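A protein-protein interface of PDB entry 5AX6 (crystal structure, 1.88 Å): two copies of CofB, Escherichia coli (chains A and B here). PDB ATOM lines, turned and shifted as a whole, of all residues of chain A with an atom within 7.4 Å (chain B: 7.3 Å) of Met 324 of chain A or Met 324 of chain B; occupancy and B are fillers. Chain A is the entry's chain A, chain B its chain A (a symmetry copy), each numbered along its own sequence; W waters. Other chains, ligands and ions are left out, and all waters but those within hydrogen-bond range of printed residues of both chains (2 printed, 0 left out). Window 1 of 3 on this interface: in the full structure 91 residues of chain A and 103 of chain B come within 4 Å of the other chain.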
ATOM      1  N   LEU A 294       1.311  10.610  -2.501  1.00  0.00           N
ATOM      2  CA  LEU A 294       0.505  11.204  -3.559  1.00  0.00           C
ATOM      3  C   LEU A 294      -0.831  11.617  -2.967  1.00  0.00           C
ATOM      4  O   LEU A 294      -1.430  10.850  -2.214  1.00  0.00           O
ATOM      5  CB  LEU A 294       0.297  10.215  -4.712  1.00  0.00           C
ATOM      6  CG  LEU A 294       1.581   9.687  -5.358  1.00  0.00           C
ATOM      7  CD1 LEU A 294       1.225   8.740  -6.497  1.00  0.00           C
ATOM      8  CD2 LEU A 294       2.429  10.861  -5.856  1.00  0.00           C
ATOM      9  N   LEU A 296      -4.790  13.417  -3.564  1.00  0.00           N
ATOM     10  CA  LEU A 296      -5.896  13.999  -4.324  1.00  0.00           C
ATOM     11  C   LEU A 296      -6.435  15.156  -3.511  1.00  0.00           C
ATOM     12  O   LEU A 296      -7.068  14.946  -2.477  1.00  0.00           O
ATOM     13  CB  LEU A 296      -7.018  12.988  -4.585  1.00  0.00           C
ATOM     14  CG  LEU A 296      -7.023  12.118  -5.830  1.00  0.00           C
ATOM     15  CD1 LEU A 296      -8.298  11.249  -5.861  1.00  0.00           C
ATOM     16  CD2 LEU A 296      -6.898  12.995  -7.074  1.00  0.00           C
ATOM     17  N   THR A 297      -6.201  16.367  -3.994  1.00  0.00           N
ATOM     18  CA  THR A 297      -6.424  17.571  -3.211  1.00  0.00           C
ATOM     19  C   THR A 297      -7.416  18.501  -3.882  1.00  0.00           C
ATOM     20  O   THR A 297      -7.374  18.677  -5.098  1.00  0.00           O
ATOM     21  CB  THR A 297      -5.106  18.316  -3.008  1.00  0.00           C
ATOM     22  OG1 THR A 297      -4.161  17.424  -2.408  1.00  0.00           O
ATOM     23  CG2 THR A 297      -5.295  19.547  -2.134  1.00  0.00           C
ATOM     24  N   SER A 310     -14.189  24.933  -7.973  1.00  0.00           N
ATOM     25  CA  SER A 310     -13.039  24.205  -7.463  1.00  0.00           C
ATOM     26  C   SER A 310     -12.785  22.997  -8.350  1.00  0.00           C
ATOM     27  O   SER A 310     -13.582  22.685  -9.230  1.00  0.00           O
ATOM     28  CB  SER A 310     -13.241  23.764  -6.001  1.00  0.00           C
ATOM     29  OG  SER A 310     -14.273  22.795  -5.891  1.00  0.00           O
ATOM     30  N   LEU A 311     -11.664  22.330  -8.103  1.00  0.00           N
ATOM     31  CA  LEU A 311     -11.332  21.114  -8.814  1.00  0.00           C
ATOM     32  C   LEU A 311     -10.470  20.255  -7.918  1.00  0.00           C
ATOM     33  O   LEU A 311     -10.055  20.681  -6.831  1.00  0.00           O
ATOM     34  CB  LEU A 311     -10.608  21.427 -10.134  1.00  0.00           C
ATOM     35  CG  LEU A 311      -9.196  22.008  -9.996  1.00  0.00           C
ATOM     36  CD1 LEU A 311      -8.374  21.686 -11.242  1.00  0.00           C
ATOM     37  CD2 LEU A 311      -9.218  23.521  -9.752  1.00  0.00           C
ATOM     38  N   ILE A 312     -10.230  19.031  -8.368  1.00  0.00           N
ATOM     39  CA  ILE A 312      -9.341  18.098  -7.687  1.00  0.00           C
ATOM     40  C   ILE A 312      -8.014  18.055  -8.427  1.00  0.00           C
ATOM     41  O   ILE A 312      -7.998  18.079  -9.660  1.00  0.00           O
ATOM     42  CB  ILE A 312      -9.920  16.673  -7.657  1.00  0.00           C
ATOM     43  CG1 ILE A 312     -11.253  16.681  -6.923  1.00  0.00           C
ATOM     44  CG2 ILE A 312      -8.920  15.720  -6.981  1.00  0.00           C
ATOM     45  CD1 ILE A 312     -11.158  17.315  -5.588  1.00  0.00           C
ATOM     46  N   LYS A 313      -6.922  17.982  -7.678  1.00  0.00           N
ATOM     47  CA  LYS A 313      -5.581  17.895  -8.264  1.00  0.00           C
ATOM     48  C   LYS A 313      -4.832  16.707  -7.666  1.00  0.00           C
ATOM     49  O   LYS A 313      -4.719  16.582  -6.442  1.00  0.00           O
ATOM     50  CB  LYS A 313      -4.806  19.202  -8.031  1.00  0.00           C
ATOM     51  CG  LYS A 313      -3.392  19.196  -8.607  1.00  0.00           C
ATOM     52  CD  LYS A 313      -2.720  20.551  -8.397  1.00  0.00           C
ATOM     53  CE  LYS A 313      -1.294  20.547  -8.949  1.00  0.00           C
ATOM     54  NZ  LYS A 313      -0.622  21.848  -8.697  1.00  0.00           N
ATOM     55  N   LEU A 314      -4.333  15.823  -8.529  1.00  0.00           N
ATOM     56  CA  LEU A 314      -3.512  14.709  -8.077  1.00  0.00           C
ATOM     57  C   LEU A 314      -2.058  15.168  -8.107  1.00  0.00           C
ATOM     58  O   LEU A 314      -1.524  15.462  -9.179  1.00  0.00           O
ATOM     59  CB  LEU A 314      -3.718  13.477  -8.968  1.00  0.00           C
ATOM     60  CG  LEU A 314      -2.913  12.226  -8.604  1.00  0.00           C
ATOM     61  CD1 LEU A 314      -3.286  11.695  -7.228  1.00  0.00           C
ATOM     62  CD2 LEU A 314      -3.118  11.139  -9.659  1.00  0.00           C
ATOM     63  N   ALA A 322       0.708  14.353 -10.477  1.00  0.00           N
ATOM     64  CA  ALA A 322       1.137  12.971 -10.474  1.00  0.00           C
ATOM     65  C   ALA A 322       0.231  12.177 -11.406  1.00  0.00           C
ATOM     66  O   ALA A 322      -0.689  12.731 -12.013  1.00  0.00           O
ATOM     67  CB  ALA A 322       1.113  12.393  -9.039  1.00  0.00           C
ATOM     68  N   THR A 323       0.495  10.882 -11.505  1.00  0.00           N
ATOM     69  CA  THR A 323      -0.113  10.028 -12.514  1.00  0.00           C
ATOM     70  C   THR A 323      -1.183   9.109 -11.985  1.00  0.00           C
ATOM     71  O   THR A 323      -1.016   8.481 -10.938  1.00  0.00           O
ATOM     72  CB  THR A 323       0.955   9.149 -13.197  1.00  0.00           C
ATOM     73  OG1 THR A 323       1.901  10.009 -13.826  1.00  0.00           O
ATOM     74  CG2 THR A 323       0.318   8.231 -14.241  1.00  0.00           C
ATOM     75  N   MET A 324      -2.279   9.035 -12.731  1.00  0.00           N
ATOM     76  CA  MET A 324      -3.306   8.030 -12.487  1.00  0.00           C
ATOM     77  C   MET A 324      -3.447   7.137 -13.719  1.00  0.00           C
ATOM     78  O   MET A 324      -3.605   7.624 -14.848  1.00  0.00           O
ATOM     79  CB  MET A 324      -4.656   8.667 -12.147  1.00  0.00           C
ATOM     80  CG  MET A 324      -5.696   7.602 -11.745  1.00  0.00           C
ATOM     81  SD  MET A 324      -7.351   8.212 -11.422  1.00  0.00           S
ATOM     82  CE  MET A 324      -7.721   9.031 -12.973  1.00  0.00           C
ATOM     83  N   LEU A 325      -3.355   5.833 -13.505  1.00  0.00           N
ATOM     84  CA  LEU A 325      -3.632   4.868 -14.567  1.00  0.00           C
ATOM     85  C   LEU A 325      -5.108   4.483 -14.483  1.00  0.00           C
ATOM     86  O   LEU A 325      -5.578   3.974 -13.466  1.00  0.00           O
ATOM     87  CB  LEU A 325      -2.710   3.647 -14.437  1.00  0.00           C
ATOM     88  CG  LEU A 325      -2.943   2.408 -15.319  1.00  0.00           C
ATOM     89  CD1 LEU A 325      -3.029   2.767 -16.770  1.00  0.00           C
ATOM     90  CD2 LEU A 325      -1.817   1.403 -15.098  1.00  0.00           C
ATOM     91  N   ALA A 326      -5.849   4.750 -15.547  1.00  0.00           N
ATOM     92  CA  ALA A 326      -7.291   4.545 -15.535  1.00  0.00           C
ATOM     93  C   ALA A 326      -7.854   4.702 -16.941  1.00  0.00           C
ATOM     94  O   ALA A 326      -7.215   5.319 -17.800  1.00  0.00           O
ATOM     95  CB  ALA A 326      -7.964   5.543 -14.590  1.00  0.00           C
ATOM     96  N   ASN A 327      -9.041   4.147 -17.172  1.00  0.00           N
ATOM     97  CA  ASN A 327      -9.842   4.523 -18.335  1.00  0.00           C
ATOM     98  C   ASN A 327     -10.616   5.784 -18.013  1.00  0.00           C
ATOM     99  O   ASN A 327     -11.222   5.881 -16.950  1.00  0.00           O
ATOM    100  CB  ASN A 327     -10.806   3.412 -18.724  1.00  0.00           C
ATOM    101  CG  ASN A 327     -10.093   2.154 -19.115  1.00  0.00           C
ATOM    102  OD1 ASN A 327      -9.064   2.203 -19.783  1.00  0.00           O
ATOM    103  ND2 ASN A 327     -10.631   1.015 -18.707  1.00  0.00           N
ATOM    104  N   ILE A 328     -10.587   6.754 -18.916  1.00  0.00           N
ATOM    105  CA  ILE A 328     -11.304   8.005 -18.683  1.00  0.00           C
ATOM    106  C   ILE A 328     -12.441   8.128 -19.659  1.00  0.00           C
ATOM    107  O   ILE A 328     -12.285   7.819 -20.837  1.00  0.00           O
ATOM    108  CB  ILE A 328     -10.392   9.245 -18.818  1.00  0.00           C
ATOM    109  CG1 ILE A 328      -9.243   9.174 -17.803  1.00  0.00           C
ATOM    110  CG2 ILE A 328     -11.221  10.534 -18.655  1.00  0.00           C
ATOM    111  CD1 ILE A 328      -9.690   9.117 -16.325  1.00  0.00           C
ATOM    112  N   LEU B 294     -17.134  18.421  -4.109  1.00  0.00           N
ATOM    113  CA  LEU B 294     -16.859  17.542  -5.238  1.00  0.00           C
ATOM    114  C   LEU B 294     -16.784  16.115  -4.723  1.00  0.00           C
ATOM    115  O   LEU B 294     -16.155  15.867  -3.696  1.00  0.00           O
ATOM    116  CB  LEU B 294     -15.549  17.931  -5.931  1.00  0.00           C
ATOM    117  CG  LEU B 294     -15.487  19.371  -6.449  1.00  0.00           C
ATOM    118  CD1 LEU B 294     -14.145  19.608  -7.133  1.00  0.00           C
ATOM    119  CD2 LEU B 294     -16.652  19.624  -7.410  1.00  0.00           C
ATOM    120  N   LEU B 296     -16.184  11.854  -5.591  1.00  0.00           N
ATOM    121  CA  LEU B 296     -15.866  10.686  -6.413  1.00  0.00           C
ATOM    122  C   LEU B 296     -16.844   9.595  -6.031  1.00  0.00           C
ATOM    123  O   LEU B 296     -16.752   9.032  -4.942  1.00  0.00           O
ATOM    124  CB  LEU B 296     -14.433  10.191  -6.192  1.00  0.00           C
ATOM    125  CG  LEU B 296     -13.280  10.713  -7.031  1.00  0.00           C
ATOM    126  CD1 LEU B 296     -11.972   9.995  -6.637  1.00  0.00           C
ATOM    127  CD2 LEU B 296     -13.602  10.541  -8.515  1.00  0.00           C
ATOM    128  N   LEU B 314     -16.560  11.636 -11.110  1.00  0.00           N
ATOM    129  CA  LEU B 314     -16.203  12.831 -10.357  1.00  0.00           C
ATOM    130  C   LEU B 314     -17.241  13.902 -10.677  1.00  0.00           C
ATOM    131  O   LEU B 314     -17.342  14.343 -11.823  1.00  0.00           O
ATOM    132  CB  LEU B 314     -14.791  13.307 -10.719  1.00  0.00           C
ATOM    133  CG  LEU B 314     -14.284  14.559  -9.997  1.00  0.00           C
ATOM    134  CD1 LEU B 314     -14.175  14.339  -8.496  1.00  0.00           C
ATOM    135  CD2 LEU B 314     -12.931  14.987 -10.565  1.00  0.00           C
ATOM    136  N   ALA B 322     -17.018  16.951 -12.817  1.00  0.00           N
ATOM    137  CA  ALA B 322     -16.100  17.968 -12.350  1.00  0.00           C
ATOM    138  C   ALA B 322     -14.701  17.630 -12.849  1.00  0.00           C
ATOM    139  O   ALA B 322     -14.504  16.624 -13.534  1.00  0.00           O
ATOM    140  CB  ALA B 322     -16.136  18.072 -10.807  1.00  0.00           C
ATOM    141  N   THR B 323     -13.741  18.472 -12.494  1.00  0.00           N
ATOM    142  CA  THR B 323     -12.405  18.431 -13.069  1.00  0.00           C
ATOM    143  C   THR B 323     -11.354  17.862 -12.153  1.00  0.00           C
ATOM    144  O   THR B 323     -11.299  18.195 -10.968  1.00  0.00           O
ATOM    145  CB  THR B 323     -11.946  19.847 -13.476  1.00  0.00           C
ATOM    146  OG1 THR B 323     -12.856  20.346 -14.452  1.00  0.00           O
ATOM    147  CG2 THR B 323     -10.532  19.814 -14.057  1.00  0.00           C
ATOM    148  N   MET B 324     -10.515  17.004 -12.725  1.00  0.00           N
ATOM    149  CA  MET B 324      -9.312  16.540 -12.046  1.00  0.00           C
ATOM    150  C   MET B 324      -8.082  16.951 -12.853  1.00  0.00           C
ATOM    151  O   MET B 324      -7.996  16.700 -14.064  1.00  0.00           O
ATOM    152  CB  MET B 324      -9.321  15.023 -11.846  1.00  0.00           C
ATOM    153  CG  MET B 324      -8.120  14.559 -10.997  1.00  0.00           C
ATOM    154  SD  MET B 324      -7.959  12.787 -10.777  1.00  0.00           S
ATOM    155  CE  MET B 324      -7.893  12.235 -12.481  1.00  0.00           C
ATOM    156  N   LEU B 325      -7.147  17.615 -12.190  1.00  0.00           N
ATOM    157  CA  LEU B 325      -5.855  17.923 -12.802  1.00  0.00           C
ATOM    158  C   LEU B 325      -4.888  16.792 -12.458  1.00  0.00           C
ATOM    159  O   LEU B 325      -4.622  16.512 -11.289  1.00  0.00           O
ATOM    160  CB  LEU B 325      -5.344  19.287 -12.317  1.00  0.00           C
ATOM    161  CG  LEU B 325      -3.917  19.743 -12.667  1.00  0.00           C
ATOM    162  CD1 LEU B 325      -3.646  19.646 -14.135  1.00  0.00           C
ATOM    163  CD2 LEU B 325      -3.707  21.177 -12.194  1.00  0.00           C
ATOM    164  N   ALA B 326      -4.377  16.122 -13.479  1.00  0.00           N
ATOM    165  CA  ALA B 326      -3.544  14.945 -13.269  1.00  0.00           C
ATOM    166  C   ALA B 326      -2.904  14.516 -14.582  1.00  0.00           C
ATOM    167  O   ALA B 326      -3.392  14.880 -15.658  1.00  0.00           O
ATOM    168  CB  ALA B 326      -4.378  13.796 -12.696  1.00  0.00           C
ATOM    169  N   ASN B 327      -1.819  13.750 -14.494  1.00  0.00           N
ATOM    170  CA  ASN B 327      -1.334  12.987 -15.641  1.00  0.00           C
ATOM    171  C   ASN B 327      -2.109  11.689 -15.732  1.00  0.00           C
ATOM    172  O   ASN B 327      -2.287  11.004 -14.729  1.00  0.00           O
ATOM    173  CB  ASN B 327       0.154  12.689 -15.517  1.00  0.00           C
ATOM    174  CG  ASN B 327       0.979  13.938 -15.484  1.00  0.00           C
ATOM    175  OD1 ASN B 327       0.701  14.889 -16.210  1.00  0.00           O
ATOM    176  ND2 ASN B 327       2.005  13.952 -14.647  1.00  0.00           N
ATOM    177  N   ILE B 328      -2.584  11.355 -16.925  1.00  0.00           N
ATOM    178  CA  ILE B 328      -3.345  10.122 -17.101  1.00  0.00           C
ATOM    179  C   ILE B 328      -2.565   9.161 -17.954  1.00  0.00           C
ATOM    180  O   ILE B 328      -1.965   9.558 -18.948  1.00  0.00           O
ATOM    181  CB  ILE B 328      -4.724  10.365 -17.754  1.00  0.00           C
ATOM    182  CG1 ILE B 328      -5.566  11.310 -16.885  1.00  0.00           C
ATOM    183  CG2 ILE B 328      -5.440   9.023 -18.000  1.00  0.00           C
ATOM    184  CD1 ILE B 328      -5.843  10.795 -15.454  1.00  0.00           C
ATOM    185  N   LEU B 329      -2.552   7.904 -17.532  1.00  0.00           N
ATOM    186  CA  LEU B 329      -2.103   6.815 -18.379  1.00  0.00           C
ATOM    187  C   LEU B 329      -3.289   5.941 -18.727  1.00  0.00           C
ATOM    188  O   LEU B 329      -4.073   5.593 -17.846  1.00  0.00           O
ATOM    189  CB  LEU B 329      -1.039   5.974 -17.678  1.00  0.00           C
ATOM    190  CG  LEU B 329       0.359   6.573 -17.657  1.00  0.00           C
ATOM    191  CD1 LEU B 329       1.323   5.622 -16.926  1.00  0.00           C
ATOM    192  CD2 LEU B 329       0.806   6.837 -19.091  1.00  0.00           C
ATOM    193  N   VAL B 330      -3.400   5.561 -19.998  1.00  0.00           N
ATOM    194  CA  VAL B 330      -4.435   4.611 -20.410  1.00  0.00           C
ATOM    195  C   VAL B 330      -3.790   3.350 -20.940  1.00  0.00           C
ATOM    196  O   VAL B 330      -2.879   3.422 -21.762  1.00  0.00           O
ATOM    197  CB  VAL B 330      -5.354   5.194 -21.495  1.00  0.00           C
ATOM    198  CG1 VAL B 330      -6.524   4.237 -21.775  1.00  0.00           C
ATOM    199  CG2 VAL B 330      -5.883   6.553 -21.058  1.00  0.00           C
ATOM    200  N   ARG B 344      -0.554   4.802 -22.953  1.00  0.00           N
ATOM    201  CA  ARG B 344      -0.463   6.100 -23.624  1.00  0.00           C
ATOM    202  C   ARG B 344      -0.957   7.215 -22.719  1.00  0.00           C
ATOM    203  O   ARG B 344      -1.705   6.967 -21.767  1.00  0.00           O
ATOM    204  CB  ARG B 344      -1.278   6.108 -24.916  1.00  0.00           C
ATOM    205  CG  ARG B 344      -2.777   6.088 -24.680  1.00  0.00           C
ATOM    206  CD  ARG B 344      -3.499   5.688 -25.952  1.00  0.00           C
ATOM    207  NE  ARG B 344      -4.946   5.735 -25.818  1.00  0.00           N
ATOM    208  CZ  ARG B 344      -5.693   4.715 -25.427  1.00  0.00           C
ATOM    209  NH1 ARG B 344      -5.120   3.560 -25.087  1.00  0.00           N
ATOM    210  NH2 ARG B 344      -7.010   4.857 -25.352  1.00  0.00           N
ATOM    211  N   VAL B 390       5.246   9.499 -14.839  1.00  0.00           N
ATOM    212  CA  VAL B 390       5.588   8.253 -14.176  1.00  0.00           C
ATOM    213  C   VAL B 390       4.793   7.101 -14.774  1.00  0.00           C
ATOM    214  O   VAL B 390       3.620   7.248 -15.107  1.00  0.00           O
ATOM    215  CB  VAL B 390       5.320   8.329 -12.649  1.00  0.00           C
ATOM    216  CG1 VAL B 390       5.520   6.976 -11.995  1.00  0.00           C
ATOM    217  CG2 VAL B 390       6.211   9.390 -11.999  1.00  0.00           C
HETATM  218  O   HOH W   1     -14.352  21.035 -11.105  1.00  0.00           O
HETATM  219  O   HOH W   2       3.868  11.808 -13.058  1.00  0.00           O
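The backbone carbonyl oxygen (O) of Thr 323 of chain B is in hydrogen-bond range of the backbone NH (N) of Ile 312 of chain A, 2.9 Å away. The backbone carbonyl oxygen (O) of Ile 312 of chain A is in hydrogen-bond range of the backbone NH (N) of Leu 325 of chain B (2.7 Å). O of Leu 325 of chain B sits at hydrogen-bond distance from N of Leu 314 of chain A. The backbone carbonyl oxygen (O) of Ala 322 of chain A sits at hydrogen-bond distance from the backbone NH (N) of Asn 327 of chain B (2.9 Å). The backbone carbonyl oxygen (O) of Val 390 of chain B is in hydrogen-bond range of the side-chain hydroxyl (OG1) of Thr 323 of chain A (3.5 Å). The backbone NH of Met 324 of chain A is in hydrogen-bond range of the backbone carbonyl oxygen of Asn 327 of chain B (2.8 Å). O of Met 324 of chain A lies within hydrogen-bond range of N of Leu 329 of chain B, 2.9 Å away. N of Ala 326 of chain A is in hydrogen-bond range of O of Leu 329 of chain B (3.0 Å).
O of Thr 297 of chain A sits at hydrogen-bond distance from N of Lys 313 of chain A (2.7 Å). The backbone carbonyl oxygen (O) of Leu 314 of chain A lies within hydrogen-bond range of the backbone NH (N) of Ala 322 of chain A, 2.8 Å away. The backbone NH (N) of Val 330 of chain B sits at hydrogen-bond distance from the backbone carbonyl oxygen (O) of Arg 344 of chain B, 2.8 Å away.
Among the printed residues, pairs that only touch across the chains: Leu 296 of chain A with Leu 296 of chain B (3.96 Å), Leu 296 of chain A with Met 324 of chain B (3.9 Å), Ser 310 of chain A with Leu 294 of chain B (3.4 Å), Leu 311 of chain A with Leu 294 of chain B (3.6 Å), Leu 311 of chain A with Thr 323 of chain B (3.4 Å), Ile 312 of chain A with Met 324 of chain B (3.1 Å), Lys 313 of chain A with Leu 325 of chain B (3.5 Å), Leu 314 of chain A with Ala 326 of chain B (3.8 Å), Ala 322 of chain A with Ala 326 of chain B (3.8 Å), Thr 323 of chain A with Asn 327 of chain B (3.3 Å), Thr 323 of chain A with Leu 329 of chain B (3.8 Å), Met 324 of chain A with Met 324 of chain B (3.2 Å), Met 324 of chain A with Ile 328 of chain B (3.4 Å), Leu 325 of chain A with Leu 329 of chain B (3.2 Å), Ala 326 of chain A with Val 330 of chain B (3.7 Å), Asn 327 of chain A with Val 330 of chain B (3.8 Å) and Ile 328 of chain A with Ile 328 of chain B (3.8 Å).
Of the printed residues of chain B, Met 324 of chain A touches Met 324, Asn 327, Ile 328 and Leu 329. Of the printed residues of chain B, Ile 328 of chain A touches Ile 328 (3.8 Å). Of the printed residues of chain B, Ala 322 of chain A touches Ala 326 and Asn 327. Of the printed residues of chain A, Leu 329 of chain B touches Thr 323, Met 324, Leu 325 and Ala 326. Of the printed residues of chain B, Leu 296 of chain A touches Leu 296 and Met 324. The nearest residue of chain A that does not touch Met 324 of chain B is Leu 314 of chain A (4.7 Å). The nearest printed residue of chain B that does not touch Lys 313 of chain A is Met 324 of chain B (4.9 Å).
Of the 15 printed residues of chain A, 13 touch a printed residue of chain B. Printed residues of chain A that touch a printed residue of chain B: Leu 296, Ser 310, Leu 311, Ile 312, Lys 313, Leu 314, Ala 322, Thr 323, Met 324, Leu 325, Ala 326, Asn 327 and Ile 328. Hydrophobic or aromatic side chains of chain A within 4 Å of the printed part of chain B: Leu 296, Leu 311, Ile 312, Leu 314, Met 324, Leu 325 and Ile 328. Hydrophobic or aromatic side chains of chain B that line the printed part of chain A: Leu 294, Leu 296, Met 324, Leu 325, Ala 326, Ile 328, Leu 329, Val 330 and Val 390. Along chain B the printed residues that touch a printed residue of chain A span positions 294 to 390. Among the printed residues, 25 pairs touch across the chains. Among the printed residues, no Asp or Glu carboxylate lies within 4 Å of a Lys or Arg side-chain nitrogen of the other chain.
Ala 322 of chain A touches Ala 326 of chain B, but with the chains exchanged Ala 326 of chain A does not touch Ala 322 of chain B (12.9 Å). Ala 322 of chain A touches Asn 327 of chain B, but with the chains exchanged Asn 327 of chain A does not touch Ala 322 of chain B (11.7 Å). Thr 323 of chain A touches Asn 327 of chain B, but with the chains exchanged Asn 327 of chain A does not touch Thr 323 of chain B (12.9 Å). Met 324 of chain A touches its own counterpart, Met 324 of chain B. Positions printed for both chains: 294, 296, 314, 322, 323, 324, 325, 326, 327 and 328. Of the 25 pairs that touch across the chains among the printed residues, 3 have their exchanged pair printed and touching as well.
Water W1 lies within hydrogen-bond range of the backbone carbonyl oxygen of Ser 310 of chain A (2.6 Å) and the backbone NH of Thr 323 of chain B (3.0 Å). Water W2 lies within hydrogen-bond range of OG1 of Thr 323 of chain A (2.8 Å), N of Val 390 of chain B (3.2 Å) and ND2 of Asn 327 of chain B (3.3 Å).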
